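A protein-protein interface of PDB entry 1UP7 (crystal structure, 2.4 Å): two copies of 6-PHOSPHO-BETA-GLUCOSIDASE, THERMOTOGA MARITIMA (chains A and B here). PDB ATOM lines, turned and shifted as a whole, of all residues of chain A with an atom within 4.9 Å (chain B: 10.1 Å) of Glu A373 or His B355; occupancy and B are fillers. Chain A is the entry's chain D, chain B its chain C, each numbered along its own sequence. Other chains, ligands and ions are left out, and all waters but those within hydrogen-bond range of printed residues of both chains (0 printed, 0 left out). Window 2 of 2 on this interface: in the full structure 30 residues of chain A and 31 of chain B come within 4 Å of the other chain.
A ring nitrogen (ND1) of His B355 sits close to the side-chain carboxylate (OE2) of Glu A373 (3.0 Å).
The backbone NH (N) of Phe B356 lies within hydrogen-bond range of the side-chain carboxylate (OD1) of Asp B354. OG of Ser B359 lies within hydrogen-bond range of O of Phe B356 (2.8 Å).
CB of Met A366 touches O of His B355, 3.4 Å away. SD of Met A366 touches CB of Leu B358 (3.6 Å). CG of Met A366 touches N of Ser B359, 3.7 Å away. Arg A369 touches His B355 (CB to ND1, 3.8 Å). His B355 touches Leu A370. N of Phe B356 touches CD1 of Leu A370, 3.6 Å away. Ser B235 touches Leu A382 (O to CD2, 3.8 Å).
Met A366 touches just these residues of chain B: His B355 (3.4 Å), Leu B358 (3.6 Å) and Ser B359 (3.7 Å). Printed residues of chain B within 4 Å of Arg A369: His B355 (3.8 Å). Leu A370 touches just these residues of chain B: His B355 and Phe B356. No residue of chain B comes within 4 Å of Ile A372. No residue of chain B comes within 4 Å of Ala A374. No residue of chain B comes within 4 Å of Lys A377. Of the printed residues of chain A, Ser B235 touches Leu A382 (3.8 Å). His B355 touches just these residues of chain A: Met A366 (3.4 Å), Arg A369 (3.8 Å), Leu A370 (3.8 Å) and Glu A373 (2.9 Å). Of the printed residues of chain A, Phe B356 touches Leu A370 (3.6 Å). Of the printed residues of chain A, Leu B358 touches Met A366. Of the printed residues of chain A, Ser B359 touches Met A366. The nearest residue of chain B that does not touch Glu A373 is Asp B354 (6.5 Å). The nearest residue of chain A that does not touch His B355 is Tyr A154 (4.7 Å). The nearest printed residue of chain B that does not touch Leu A382 is Arg B237 (5.8 Å).
Printed residues of chain A that touch a printed residue of chain B: Met A366, Arg A369, Leu A370, Glu A373 and Leu A382. Of the 23 printed residues of chain B, 5 touch a printed residue of chain A. Printed residues of chain B that touch a printed residue of chain A: Ser B235, His B355, Phe B356, Leu B358 and Ser B359. Among the printed residues, 8 pairs touch across the chains. Among the printed residues, no Asp or Glu carboxylate lies within 4 Å of a Lys or Arg side-chain nitrogen of the other chain.
No position is printed for both chains.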
ATOM      1  N   TYR A 154      35.694 -19.964  23.319  1.00  0.00           N
ATOM      2  CA  TYR A 154      36.779 -20.883  22.958  1.00  0.00           C
ATOM      3  C   TYR A 154      37.918 -20.835  23.959  1.00  0.00           C
ATOM      4  O   TYR A 154      38.387 -21.873  24.423  1.00  0.00           O
ATOM      5  CB  TYR A 154      37.248 -20.633  21.513  1.00  0.00           C
ATOM      6  CG  TYR A 154      36.145 -20.915  20.523  1.00  0.00           C
ATOM      7  CD1 TYR A 154      35.192 -19.944  20.211  1.00  0.00           C
ATOM      8  CD2 TYR A 154      36.041 -22.174  19.926  1.00  0.00           C
ATOM      9  CE1 TYR A 154      34.159 -20.214  19.316  1.00  0.00           C
ATOM     10  CE2 TYR A 154      35.040 -22.462  19.044  1.00  0.00           C
ATOM     11  CZ  TYR A 154      34.095 -21.482  18.734  1.00  0.00           C
ATOM     12  OH  TYR A 154      33.111 -21.799  17.841  1.00  0.00           O
ATOM     13  N   MET A 366      27.982 -17.788  12.170  1.00  0.00           N
ATOM     14  CA  MET A 366      28.488 -19.049  11.629  1.00  0.00           C
ATOM     15  C   MET A 366      29.860 -18.852  11.028  1.00  0.00           C
ATOM     16  O   MET A 366      30.803 -19.629  11.323  1.00  0.00           O
ATOM     17  CB  MET A 366      27.521 -19.665  10.597  1.00  0.00           C
ATOM     18  CG  MET A 366      26.152 -20.072  11.167  1.00  0.00           C
ATOM     19  SD  MET A 366      26.217 -21.314  12.529  1.00  0.00           S
ATOM     20  CE  MET A 366      26.180 -20.211  13.977  1.00  0.00           C
ATOM     21  N   ARG A 369      32.525 -18.493  13.800  1.00  0.00           N
ATOM     22  CA  ARG A 369      32.965 -19.726  14.432  1.00  0.00           C
ATOM     23  C   ARG A 369      33.840 -20.573  13.517  1.00  0.00           C
ATOM     24  O   ARG A 369      34.753 -21.244  13.995  1.00  0.00           O
ATOM     25  CB  ARG A 369      31.798 -20.529  14.993  1.00  0.00           C
ATOM     26  CG  ARG A 369      30.755 -19.654  15.628  1.00  0.00           C
ATOM     27  CD  ARG A 369      30.537 -19.858  17.095  1.00  0.00           C
ATOM     28  NE  ARG A 369      29.258 -20.469  17.346  1.00  0.00           N
ATOM     29  CZ  ARG A 369      28.389 -20.088  18.296  1.00  0.00           C
ATOM     30  NH1 ARG A 369      28.634 -19.074  19.111  1.00  0.00           N
ATOM     31  NH2 ARG A 369      27.259 -20.751  18.434  1.00  0.00           N
ATOM     32  N   LEU A 370      33.561 -20.508  12.217  1.00  0.00           N
ATOM     33  CA  LEU A 370      34.321 -21.235  11.207  1.00  0.00           C
ATOM     34  C   LEU A 370      35.742 -20.679  11.083  1.00  0.00           C
ATOM     35  O   LEU A 370      36.687 -21.430  10.854  1.00  0.00           O
ATOM     36  CB  LEU A 370      33.616 -21.169   9.839  1.00  0.00           C
ATOM     37  CG  LEU A 370      32.380 -22.075   9.663  1.00  0.00           C
ATOM     38  CD1 LEU A 370      31.628 -21.700   8.360  1.00  0.00           C
ATOM     39  CD2 LEU A 370      32.735 -23.578   9.701  1.00  0.00           C
ATOM     40  N   THR A 371      35.848 -19.357  11.217  1.00  0.00           N
ATOM     41  CA  THR A 371      37.112 -18.638  11.243  1.00  0.00           C
ATOM     42  C   THR A 371      37.935 -19.029  12.477  1.00  0.00           C
ATOM     43  O   THR A 371      39.121 -19.320  12.370  1.00  0.00           O
ATOM     44  CB  THR A 371      36.842 -17.107  11.187  1.00  0.00           C
ATOM     45  OG1 THR A 371      36.196 -16.792   9.945  1.00  0.00           O
ATOM     46  CG2 THR A 371      38.118 -16.314  11.092  1.00  0.00           C
ATOM     47  N   ILE A 372      37.280 -19.040  13.637  1.00  0.00           N
ATOM     48  CA  ILE A 372      37.930 -19.454  14.876  1.00  0.00           C
ATOM     49  C   ILE A 372      38.407 -20.913  14.766  1.00  0.00           C
ATOM     50  O   ILE A 372      39.536 -21.239  15.150  1.00  0.00           O
ATOM     51  CB  ILE A 372      36.980 -19.215  16.077  1.00  0.00           C
ATOM     52  CG1 ILE A 372      36.876 -17.719  16.366  1.00  0.00           C
ATOM     53  CG2 ILE A 372      37.456 -19.920  17.345  1.00  0.00           C
ATOM     54  CD1 ILE A 372      35.616 -17.352  17.132  1.00  0.00           C
ATOM     55  N   GLU A 373      37.544 -21.764  14.221  1.00  0.00           N
ATOM     56  CA  GLU A 373      37.844 -23.183  14.075  1.00  0.00           C
ATOM     57  C   GLU A 373      39.042 -23.344  13.133  1.00  0.00           C
ATOM     58  O   GLU A 373      39.941 -24.110  13.413  1.00  0.00           O
ATOM     59  CB  GLU A 373      36.601 -23.980  13.599  1.00  0.00           C
ATOM     60  CG  GLU A 373      35.613 -24.377  14.713  1.00  0.00           C
ATOM     61  CD  GLU A 373      34.126 -24.450  14.265  1.00  0.00           C
ATOM     62  OE1 GLU A 373      33.815 -24.776  13.072  1.00  0.00           O
ATOM     63  OE2 GLU A 373      33.238 -24.175  15.130  1.00  0.00           O
ATOM     64  N   ALA A 374      39.068 -22.585  12.041  1.00  0.00           N
ATOM     65  CA  ALA A 374      40.206 -22.620  11.113  1.00  0.00           C
ATOM     66  C   ALA A 374      41.503 -22.267  11.827  1.00  0.00           C
ATOM     67  O   ALA A 374      42.509 -22.952  11.649  1.00  0.00           O
ATOM     68  CB  ALA A 374      39.988 -21.691   9.933  1.00  0.00           C
ATOM     69  N   TYR A 375      41.444 -21.211  12.636  1.00  0.00           N
ATOM     70  CA  TYR A 375      42.579 -20.727  13.398  1.00  0.00           C
ATOM     71  C   TYR A 375      43.113 -21.753  14.404  1.00  0.00           C
ATOM     72  O   TYR A 375      44.320 -22.002  14.435  1.00  0.00           O
ATOM     73  CB  TYR A 375      42.265 -19.367  14.076  1.00  0.00           C
ATOM     74  CG  TYR A 375      43.311 -19.022  15.097  1.00  0.00           C
ATOM     75  CD1 TYR A 375      44.600 -18.588  14.701  1.00  0.00           C
ATOM     76  CD2 TYR A 375      43.074 -19.234  16.441  1.00  0.00           C
ATOM     77  CE1 TYR A 375      45.584 -18.325  15.643  1.00  0.00           C
ATOM     78  CE2 TYR A 375      44.049 -18.978  17.385  1.00  0.00           C
ATOM     79  CZ  TYR A 375      45.296 -18.524  16.993  1.00  0.00           C
ATOM     80  OH  TYR A 375      46.254 -18.287  17.966  1.00  0.00           O
ATOM     81  N   LEU A 376      42.230 -22.341  15.215  1.00  0.00           N
ATOM     82  CA  LEU A 376      42.626 -23.287  16.268  1.00  0.00           C
ATOM     83  C   LEU A 376      43.282 -24.559  15.710  1.00  0.00           C
ATOM     84  O   LEU A 376      44.155 -25.178  16.368  1.00  0.00           O
ATOM     85  CB  LEU A 376      41.433 -23.676  17.137  1.00  0.00           C
ATOM     86  CG  LEU A 376      40.874 -22.606  18.068  1.00  0.00           C
ATOM     87  CD1 LEU A 376      39.466 -22.973  18.553  1.00  0.00           C
ATOM     88  CD2 LEU A 376      41.808 -22.383  19.252  1.00  0.00           C
ATOM     89  N   LYS A 377      42.863 -24.928  14.495  1.00  0.00           N
ATOM     90  CA  LYS A 377      43.451 -26.048  13.785  1.00  0.00           C
ATOM     91  C   LYS A 377      44.544 -25.596  12.806  1.00  0.00           C
ATOM     92  O   LYS A 377      45.104 -26.415  12.069  1.00  0.00           O
ATOM     93  CB  LYS A 377      42.357 -26.819  13.060  1.00  0.00           C
ATOM     94  CG  LYS A 377      41.886 -28.038  13.846  1.00  0.00           C
ATOM     95  CD  LYS A 377      40.397 -28.067  13.976  1.00  0.00           C
ATOM     96  CE  LYS A 377      39.900 -29.508  14.026  1.00  0.00           C
ATOM     97  NZ  LYS A 377      38.419 -29.600  13.887  1.00  0.00           N
ATOM     98  N   LEU A 382      40.264 -25.307   6.313  1.00  0.00           N
ATOM     99  CA  LEU A 382      39.168 -24.751   7.083  1.00  0.00           C
ATOM    100  C   LEU A 382      39.044 -23.241   6.933  1.00  0.00           C
ATOM    101  O   LEU A 382      37.939 -22.706   7.068  1.00  0.00           O
ATOM    102  CB  LEU A 382      39.250 -25.171   8.551  1.00  0.00           C
ATOM    103  CG  LEU A 382      39.084 -26.683   8.716  1.00  0.00           C
ATOM    104  CD1 LEU A 382      39.375 -27.074  10.154  1.00  0.00           C
ATOM    105  CD2 LEU A 382      37.711 -27.200   8.247  1.00  0.00           C
ATOM    106  N   LYS B 188      23.463 -38.915   6.452  1.00  0.00           N
ATOM    107  CA  LYS B 188      23.275 -37.739   7.285  1.00  0.00           C
ATOM    108  C   LYS B 188      23.102 -36.579   6.317  1.00  0.00           C
ATOM    109  O   LYS B 188      24.045 -36.158   5.633  1.00  0.00           O
ATOM    110  CB  LYS B 188      24.398 -37.507   8.282  1.00  0.00           C
ATOM    111  CG  LYS B 188      24.111 -36.314   9.201  1.00  0.00           C
ATOM    112  CD  LYS B 188      25.238 -36.065  10.241  1.00  0.00           C
ATOM    113  CE  LYS B 188      24.957 -34.744  10.947  1.00  0.00           C
ATOM    114  NZ  LYS B 188      25.724 -34.608  12.201  1.00  0.00           N
ATOM    115  N   TYR B 190      20.765 -32.901   5.571  1.00  0.00           N
ATOM    116  CA  TYR B 190      19.941 -31.829   6.125  1.00  0.00           C
ATOM    117  C   TYR B 190      20.117 -30.544   5.348  1.00  0.00           C
ATOM    118  O   TYR B 190      21.105 -30.343   4.653  1.00  0.00           O
ATOM    119  CB  TYR B 190      20.239 -31.567   7.619  1.00  0.00           C
ATOM    120  CG  TYR B 190      21.685 -31.270   7.882  1.00  0.00           C
ATOM    121  CD1 TYR B 190      22.617 -32.302   8.003  1.00  0.00           C
ATOM    122  CD2 TYR B 190      22.134 -29.963   7.971  1.00  0.00           C
ATOM    123  CE1 TYR B 190      23.943 -32.035   8.194  1.00  0.00           C
ATOM    124  CE2 TYR B 190      23.459 -29.696   8.194  1.00  0.00           C
ATOM    125  CZ  TYR B 190      24.359 -30.736   8.303  1.00  0.00           C
ATOM    126  OH  TYR B 190      25.684 -30.458   8.505  1.00  0.00           O
ATOM    127  N   PHE B 197      22.675 -30.504   2.323  1.00  0.00           N
ATOM    128  CA  PHE B 197      24.047 -30.872   2.580  1.00  0.00           C
ATOM    129  C   PHE B 197      24.073 -32.327   3.021  1.00  0.00           C
ATOM    130  O   PHE B 197      23.186 -32.778   3.765  1.00  0.00           O
ATOM    131  CB  PHE B 197      24.591 -29.961   3.686  1.00  0.00           C
ATOM    132  CG  PHE B 197      24.538 -28.524   3.323  1.00  0.00           C
ATOM    133  CD1 PHE B 197      23.382 -27.763   3.568  1.00  0.00           C
ATOM    134  CD2 PHE B 197      25.604 -27.938   2.647  1.00  0.00           C
ATOM    135  CE1 PHE B 197      23.321 -26.424   3.183  1.00  0.00           C
ATOM    136  CE2 PHE B 197      25.562 -26.611   2.267  1.00  0.00           C
ATOM    137  CZ  PHE B 197      24.437 -25.846   2.520  1.00  0.00           C
ATOM    138  N   GLU B 199      26.556 -34.936   4.965  1.00  0.00           N
ATOM    139  CA  GLU B 199      27.726 -34.992   5.803  1.00  0.00           C
ATOM    140  C   GLU B 199      28.314 -36.400   5.915  1.00  0.00           C
ATOM    141  O   GLU B 199      29.503 -36.547   6.039  1.00  0.00           O
ATOM    142  CB  GLU B 199      27.383 -34.413   7.153  1.00  0.00           C
ATOM    143  CG  GLU B 199      28.585 -33.789   7.834  1.00  0.00           C
ATOM    144  CD  GLU B 199      28.218 -33.187   9.166  1.00  0.00           C
ATOM    145  OE1 GLU B 199      27.099 -32.630   9.306  1.00  0.00           O
ATOM    146  OE2 GLU B 199      29.057 -33.290  10.073  1.00  0.00           O
ATOM    147  N   SER B 235      37.949 -28.863   1.718  1.00  0.00           N
ATOM    148  CA  SER B 235      37.825 -27.722   2.627  1.00  0.00           C
ATOM    149  C   SER B 235      36.544 -27.777   3.423  1.00  0.00           C
ATOM    150  O   SER B 235      36.555 -27.719   4.642  1.00  0.00           O
ATOM    151  CB  SER B 235      37.782 -26.412   1.825  1.00  0.00           C
ATOM    152  OG  SER B 235      39.079 -26.045   1.411  1.00  0.00           O
ATOM    153  N   VAL B 236      35.443 -27.883   2.693  1.00  0.00           N
ATOM    154  CA  VAL B 236      34.117 -27.747   3.259  1.00  0.00           C
ATOM    155  C   VAL B 236      33.663 -29.062   3.890  1.00  0.00           C
ATOM    156  O   VAL B 236      32.899 -29.046   4.867  1.00  0.00           O
ATOM    157  CB  VAL B 236      33.088 -27.233   2.201  1.00  0.00           C
ATOM    158  CG1 VAL B 236      31.667 -27.280   2.728  1.00  0.00           C
ATOM    159  CG2 VAL B 236      33.430 -25.812   1.734  1.00  0.00           C
ATOM    160  N   ARG B 237      34.155 -30.177   3.335  1.00  0.00           N
ATOM    161  CA  ARG B 237      33.810 -31.548   3.769  1.00  0.00           C
ATOM    162  C   ARG B 237      32.316 -31.843   3.850  1.00  0.00           C
ATOM    163  O   ARG B 237      31.868 -32.553   4.717  1.00  0.00           O
ATOM    164  CB  ARG B 237      34.533 -31.937   5.054  1.00  0.00           C
ATOM    165  CG  ARG B 237      36.006 -32.338   4.785  1.00  0.00           C
ATOM    166  CD  ARG B 237      36.837 -32.540   6.046  1.00  0.00           C
ATOM    167  NE  ARG B 237      37.138 -33.967   6.252  1.00  0.00           N
ATOM    168  CZ  ARG B 237      36.358 -34.815   6.936  1.00  0.00           C
ATOM    169  NH1 ARG B 237      35.228 -34.390   7.503  1.00  0.00           N
ATOM    170  NH2 ARG B 237      36.718 -36.089   7.067  1.00  0.00           N
ATOM    171  N   LEU B 238      31.561 -31.278   2.921  1.00  0.00           N
ATOM    172  CA  LEU B 238      30.155 -31.580   2.750  1.00  0.00           C
ATOM    173  C   LEU B 238      29.886 -31.836   1.281  1.00  0.00           C
ATOM    174  O   LEU B 238      30.464 -31.197   0.415  1.00  0.00           O
ATOM    175  CB  LEU B 238      29.271 -30.415   3.205  1.00  0.00           C
ATOM    176  CG  LEU B 238      29.373 -30.012   4.675  1.00  0.00           C
ATOM    177  CD1 LEU B 238      28.686 -28.688   4.916  1.00  0.00           C
ATOM    178  CD2 LEU B 238      28.759 -31.088   5.573  1.00  0.00           C
ATOM    179  N   ILE B 325      18.180 -32.165  13.688  1.00  0.00           N
ATOM    180  CA  ILE B 325      19.403 -31.399  13.784  1.00  0.00           C
ATOM    181  C   ILE B 325      19.327 -30.602  15.089  1.00  0.00           C
ATOM    182  O   ILE B 325      18.553 -29.644  15.209  1.00  0.00           O
ATOM    183  CB  ILE B 325      19.578 -30.467  12.534  1.00  0.00           C
ATOM    184  CG1 ILE B 325      19.823 -31.297  11.267  1.00  0.00           C
ATOM    185  CG2 ILE B 325      20.753 -29.502  12.749  1.00  0.00           C
ATOM    186  CD1 ILE B 325      21.199 -32.138  11.288  1.00  0.00           C
ATOM    187  N   ASN B 327      21.175 -28.391  16.659  1.00  0.00           N
ATOM    188  CA  ASN B 327      21.508 -26.963  16.757  1.00  0.00           C
ATOM    189  C   ASN B 327      20.720 -26.104  15.770  1.00  0.00           C
ATOM    190  O   ASN B 327      21.186 -25.062  15.336  1.00  0.00           O
ATOM    191  CB  ASN B 327      23.018 -26.703  16.633  1.00  0.00           C
ATOM    192  CG  ASN B 327      23.636 -27.335  15.376  1.00  0.00           C
ATOM    193  OD1 ASN B 327      23.016 -28.171  14.720  1.00  0.00           O
ATOM    194  ND2 ASN B 327      24.885 -26.958  15.065  1.00  0.00           N
ATOM    195  N   LEU B 328      19.537 -26.570  15.396  1.00  0.00           N
ATOM    196  CA  LEU B 328      18.603 -25.779  14.601  1.00  0.00           C
ATOM    197  C   LEU B 328      17.299 -25.847  15.379  1.00  0.00           C
ATOM    198  O   LEU B 328      17.052 -26.850  16.050  1.00  0.00           O
ATOM    199  CB  LEU B 328      18.400 -26.385  13.202  1.00  0.00           C
ATOM    200  CG  LEU B 328      18.909 -25.682  11.941  1.00  0.00           C
ATOM    201  CD1 LEU B 328      19.763 -24.444  12.224  1.00  0.00           C
ATOM    202  CD2 LEU B 328      19.587 -26.635  10.988  1.00  0.00           C
ATOM    203  N   LYS B 352      24.575 -32.732  15.288  1.00  0.00           N
ATOM    204  CA  LYS B 352      24.746 -31.309  14.974  1.00  0.00           C
ATOM    205  C   LYS B 352      24.914 -31.045  13.478  1.00  0.00           C
ATOM    206  O   LYS B 352      25.555 -31.809  12.764  1.00  0.00           O
ATOM    207  CB  LYS B 352      25.988 -30.719  15.680  1.00  0.00           C
ATOM    208  CG  LYS B 352      25.969 -30.842  17.189  1.00  0.00           C
ATOM    209  CD  LYS B 352      26.837 -29.782  17.845  1.00  0.00           C
ATOM    210  CE  LYS B 352      27.009 -30.059  19.353  1.00  0.00           C
ATOM    211  NZ  LYS B 352      28.437 -29.894  19.841  1.00  0.00           N
ATOM    212  N   GLY B 353      24.379 -29.925  13.031  1.00  0.00           N
ATOM    213  CA  GLY B 353      24.645 -29.436  11.693  1.00  0.00           C
ATOM    214  C   GLY B 353      25.926 -28.617  11.659  1.00  0.00           C
ATOM    215  O   GLY B 353      26.291 -27.944  12.628  1.00  0.00           O
ATOM    216  N   ASP B 354      26.603 -28.688  10.519  1.00  0.00           N
ATOM    217  CA  ASP B 354      27.852 -27.979  10.269  1.00  0.00           C
ATOM    218  C   ASP B 354      27.552 -26.456  10.156  1.00  0.00           C
ATOM    219  O   ASP B 354      26.562 -26.076   9.547  1.00  0.00           O
ATOM    220  CB  ASP B 354      28.464 -28.547   8.981  1.00  0.00           C
ATOM    221  CG  ASP B 354      29.806 -27.957   8.656  1.00  0.00           C
ATOM    222  OD1 ASP B 354      29.893 -26.753   8.340  1.00  0.00           O
ATOM    223  OD2 ASP B 354      30.844 -28.625   8.653  1.00  0.00           O
ATOM    224  N   HIS B 355      28.388 -25.616  10.766  1.00  0.00           N
ATOM    225  CA  HIS B 355      28.229 -24.164  10.735  1.00  0.00           C
ATOM    226  C   HIS B 355      28.138 -23.600   9.313  1.00  0.00           C
ATOM    227  O   HIS B 355      27.388 -22.665   9.068  1.00  0.00           O
ATOM    228  CB  HIS B 355      29.384 -23.466  11.472  1.00  0.00           C
ATOM    229  CG  HIS B 355      29.422 -23.749  12.938  1.00  0.00           C
ATOM    230  ND1 HIS B 355      30.601 -23.844  13.648  1.00  0.00           N
ATOM    231  CD2 HIS B 355      28.424 -23.977  13.826  1.00  0.00           C
ATOM    232  CE1 HIS B 355      30.325 -24.130  14.907  1.00  0.00           C
ATOM    233  NE2 HIS B 355      29.013 -24.210  15.040  1.00  0.00           N
ATOM    234  N   PHE B 356      28.927 -24.150   8.389  1.00  0.00           N
ATOM    235  CA  PHE B 356      28.873 -23.727   6.985  1.00  0.00           C
ATOM    236  C   PHE B 356      27.462 -23.932   6.443  1.00  0.00           C
ATOM    237  O   PHE B 356      26.908 -23.024   5.814  1.00  0.00           O
ATOM    238  CB  PHE B 356      29.883 -24.499   6.128  1.00  0.00           C
ATOM    239  CG  PHE B 356      29.940 -24.062   4.683  1.00  0.00           C
ATOM    240  CD1 PHE B 356      29.103 -24.631   3.739  1.00  0.00           C
ATOM    241  CD2 PHE B 356      30.877 -23.113   4.268  1.00  0.00           C
ATOM    242  CE1 PHE B 356      29.152 -24.228   2.385  1.00  0.00           C
ATOM    243  CE2 PHE B 356      30.954 -22.695   2.941  1.00  0.00           C
ATOM    244  CZ  PHE B 356      30.106 -23.245   1.986  1.00  0.00           C
ATOM    245  N   ALA B 357      26.888 -25.116   6.691  1.00  0.00           N
ATOM    246  CA  ALA B 357      25.522 -25.413   6.252  1.00  0.00           C
ATOM    247  C   ALA B 357      24.522 -24.495   6.951  1.00  0.00           C
ATOM    248  O   ALA B 357      23.608 -23.955   6.308  1.00  0.00           O
ATOM    249  CB  ALA B 357      25.156 -26.880   6.480  1.00  0.00           C
ATOM    250  N   LEU B 358      24.701 -24.300   8.258  1.00  0.00           N
ATOM    251  CA  LEU B 358      23.818 -23.401   9.014  1.00  0.00           C
ATOM    252  C   LEU B 358      23.819 -21.945   8.524  1.00  0.00           C
ATOM    253  O   LEU B 358      22.790 -21.272   8.606  1.00  0.00           O
ATOM    254  CB  LEU B 358      24.115 -23.481  10.498  1.00  0.00           C
ATOM    255  CG  LEU B 358      23.195 -24.461  11.251  1.00  0.00           C
ATOM    256  CD1 LEU B 358      23.212 -25.901  10.732  1.00  0.00           C
ATOM    257  CD2 LEU B 358      23.524 -24.417  12.726  1.00  0.00           C
ATOM    258  N   SER B 359      24.945 -21.460   7.994  1.00  0.00           N
ATOM    259  CA  SER B 359      24.975 -20.095   7.521  1.00  0.00           C
ATOM    260  C   SER B 359      23.937 -19.899   6.429  1.00  0.00           C
ATOM    261  O   SER B 359      23.269 -18.873   6.416  1.00  0.00           O
ATOM    262  CB  SER B 359      26.357 -19.656   7.050  1.00  0.00           C
ATOM    263  OG  SER B 359      26.663 -20.185   5.781  1.00  0.00           O
ATOM    264  N   PHE B 360      23.779 -20.884   5.544  1.00  0.00           N
ATOM    265  CA  PHE B 360      22.786 -20.813   4.474  1.00  0.00           C
ATOM    266  C   PHE B 360      21.372 -21.107   4.986  1.00  0.00           C
ATOM    267  O   PHE B 360      20.423 -20.375   4.706  1.00  0.00           O
ATOM    268  CB  PHE B 360      23.111 -21.784   3.307  1.00  0.00           C
ATOM    269  CG  PHE B 360      24.353 -21.447   2.567  1.00  0.00           C
ATOM    270  CD1 PHE B 360      24.332 -20.512   1.542  1.00  0.00           C
ATOM    271  CD2 PHE B 360      25.554 -22.060   2.901  1.00  0.00           C
ATOM    272  CE1 PHE B 360      25.518 -20.176   0.850  1.00  0.00           C
ATOM    273  CE2 PHE B 360      26.745 -21.748   2.218  1.00  0.00           C
ATOM    274  CZ  PHE B 360      26.720 -20.814   1.191  1.00  0.00           C
ATOM    275  N   ILE B 361      21.224 -22.195   5.715  1.00  0.00           N
ATOM    276  CA  ILE B 361      19.919 -22.610   6.200  1.00  0.00           C
ATOM    277  C   ILE B 361      19.203 -21.498   6.976  1.00  0.00           C
ATOM    278  O   ILE B 361      18.034 -21.209   6.676  1.00  0.00           O
ATOM    279  CB  ILE B 361      20.064 -23.879   7.083  1.00  0.00           C
ATOM    280  CG1 ILE B 361      20.568 -25.068   6.226  1.00  0.00           C
ATOM    281  CG2 ILE B 361      18.741 -24.174   7.778  1.00  0.00           C
ATOM    282  CD1 ILE B 361      21.051 -26.252   7.055  1.00  0.00           C
ATOM    283  N   HIS B 362      19.888 -20.895   7.967  1.00  0.00           N
ATOM    284  CA  HIS B 362      19.313 -19.782   8.748  1.00  0.00           C
ATOM    285  C   HIS B 362      18.922 -18.578   7.859  1.00  0.00           C
ATOM    286  O   HIS B 362      17.830 -18.038   7.992  1.00  0.00           O
ATOM    287  CB  HIS B 362      20.292 -19.257   9.778  1.00  0.00           C
ATOM    288  CG  HIS B 362      20.380 -20.055  11.039  1.00  0.00           C
ATOM    289  ND1 HIS B 362      19.281 -20.326  11.833  1.00  0.00           N
ATOM    290  CD2 HIS B 362      21.459 -20.543  11.703  1.00  0.00           C
ATOM    291  CE1 HIS B 362      19.676 -20.988  12.907  1.00  0.00           C
ATOM    292  NE2 HIS B 362      20.994 -21.126  12.851  1.00  0.00           N
ATOM    293  N   ALA B 363      19.832 -18.126   6.989  1.00  0.00           N
ATOM    294  CA  ALA B 363      19.553 -16.933   6.205  1.00  0.00           C
ATOM    295  C   ALA B 363      18.331 -17.157   5.318  1.00  0.00           C
ATOM    296  O   ALA B 363      17.458 -16.280   5.212  1.00  0.00           O
ATOM    297  CB  ALA B 363      20.745 -16.513   5.362  1.00  0.00           C
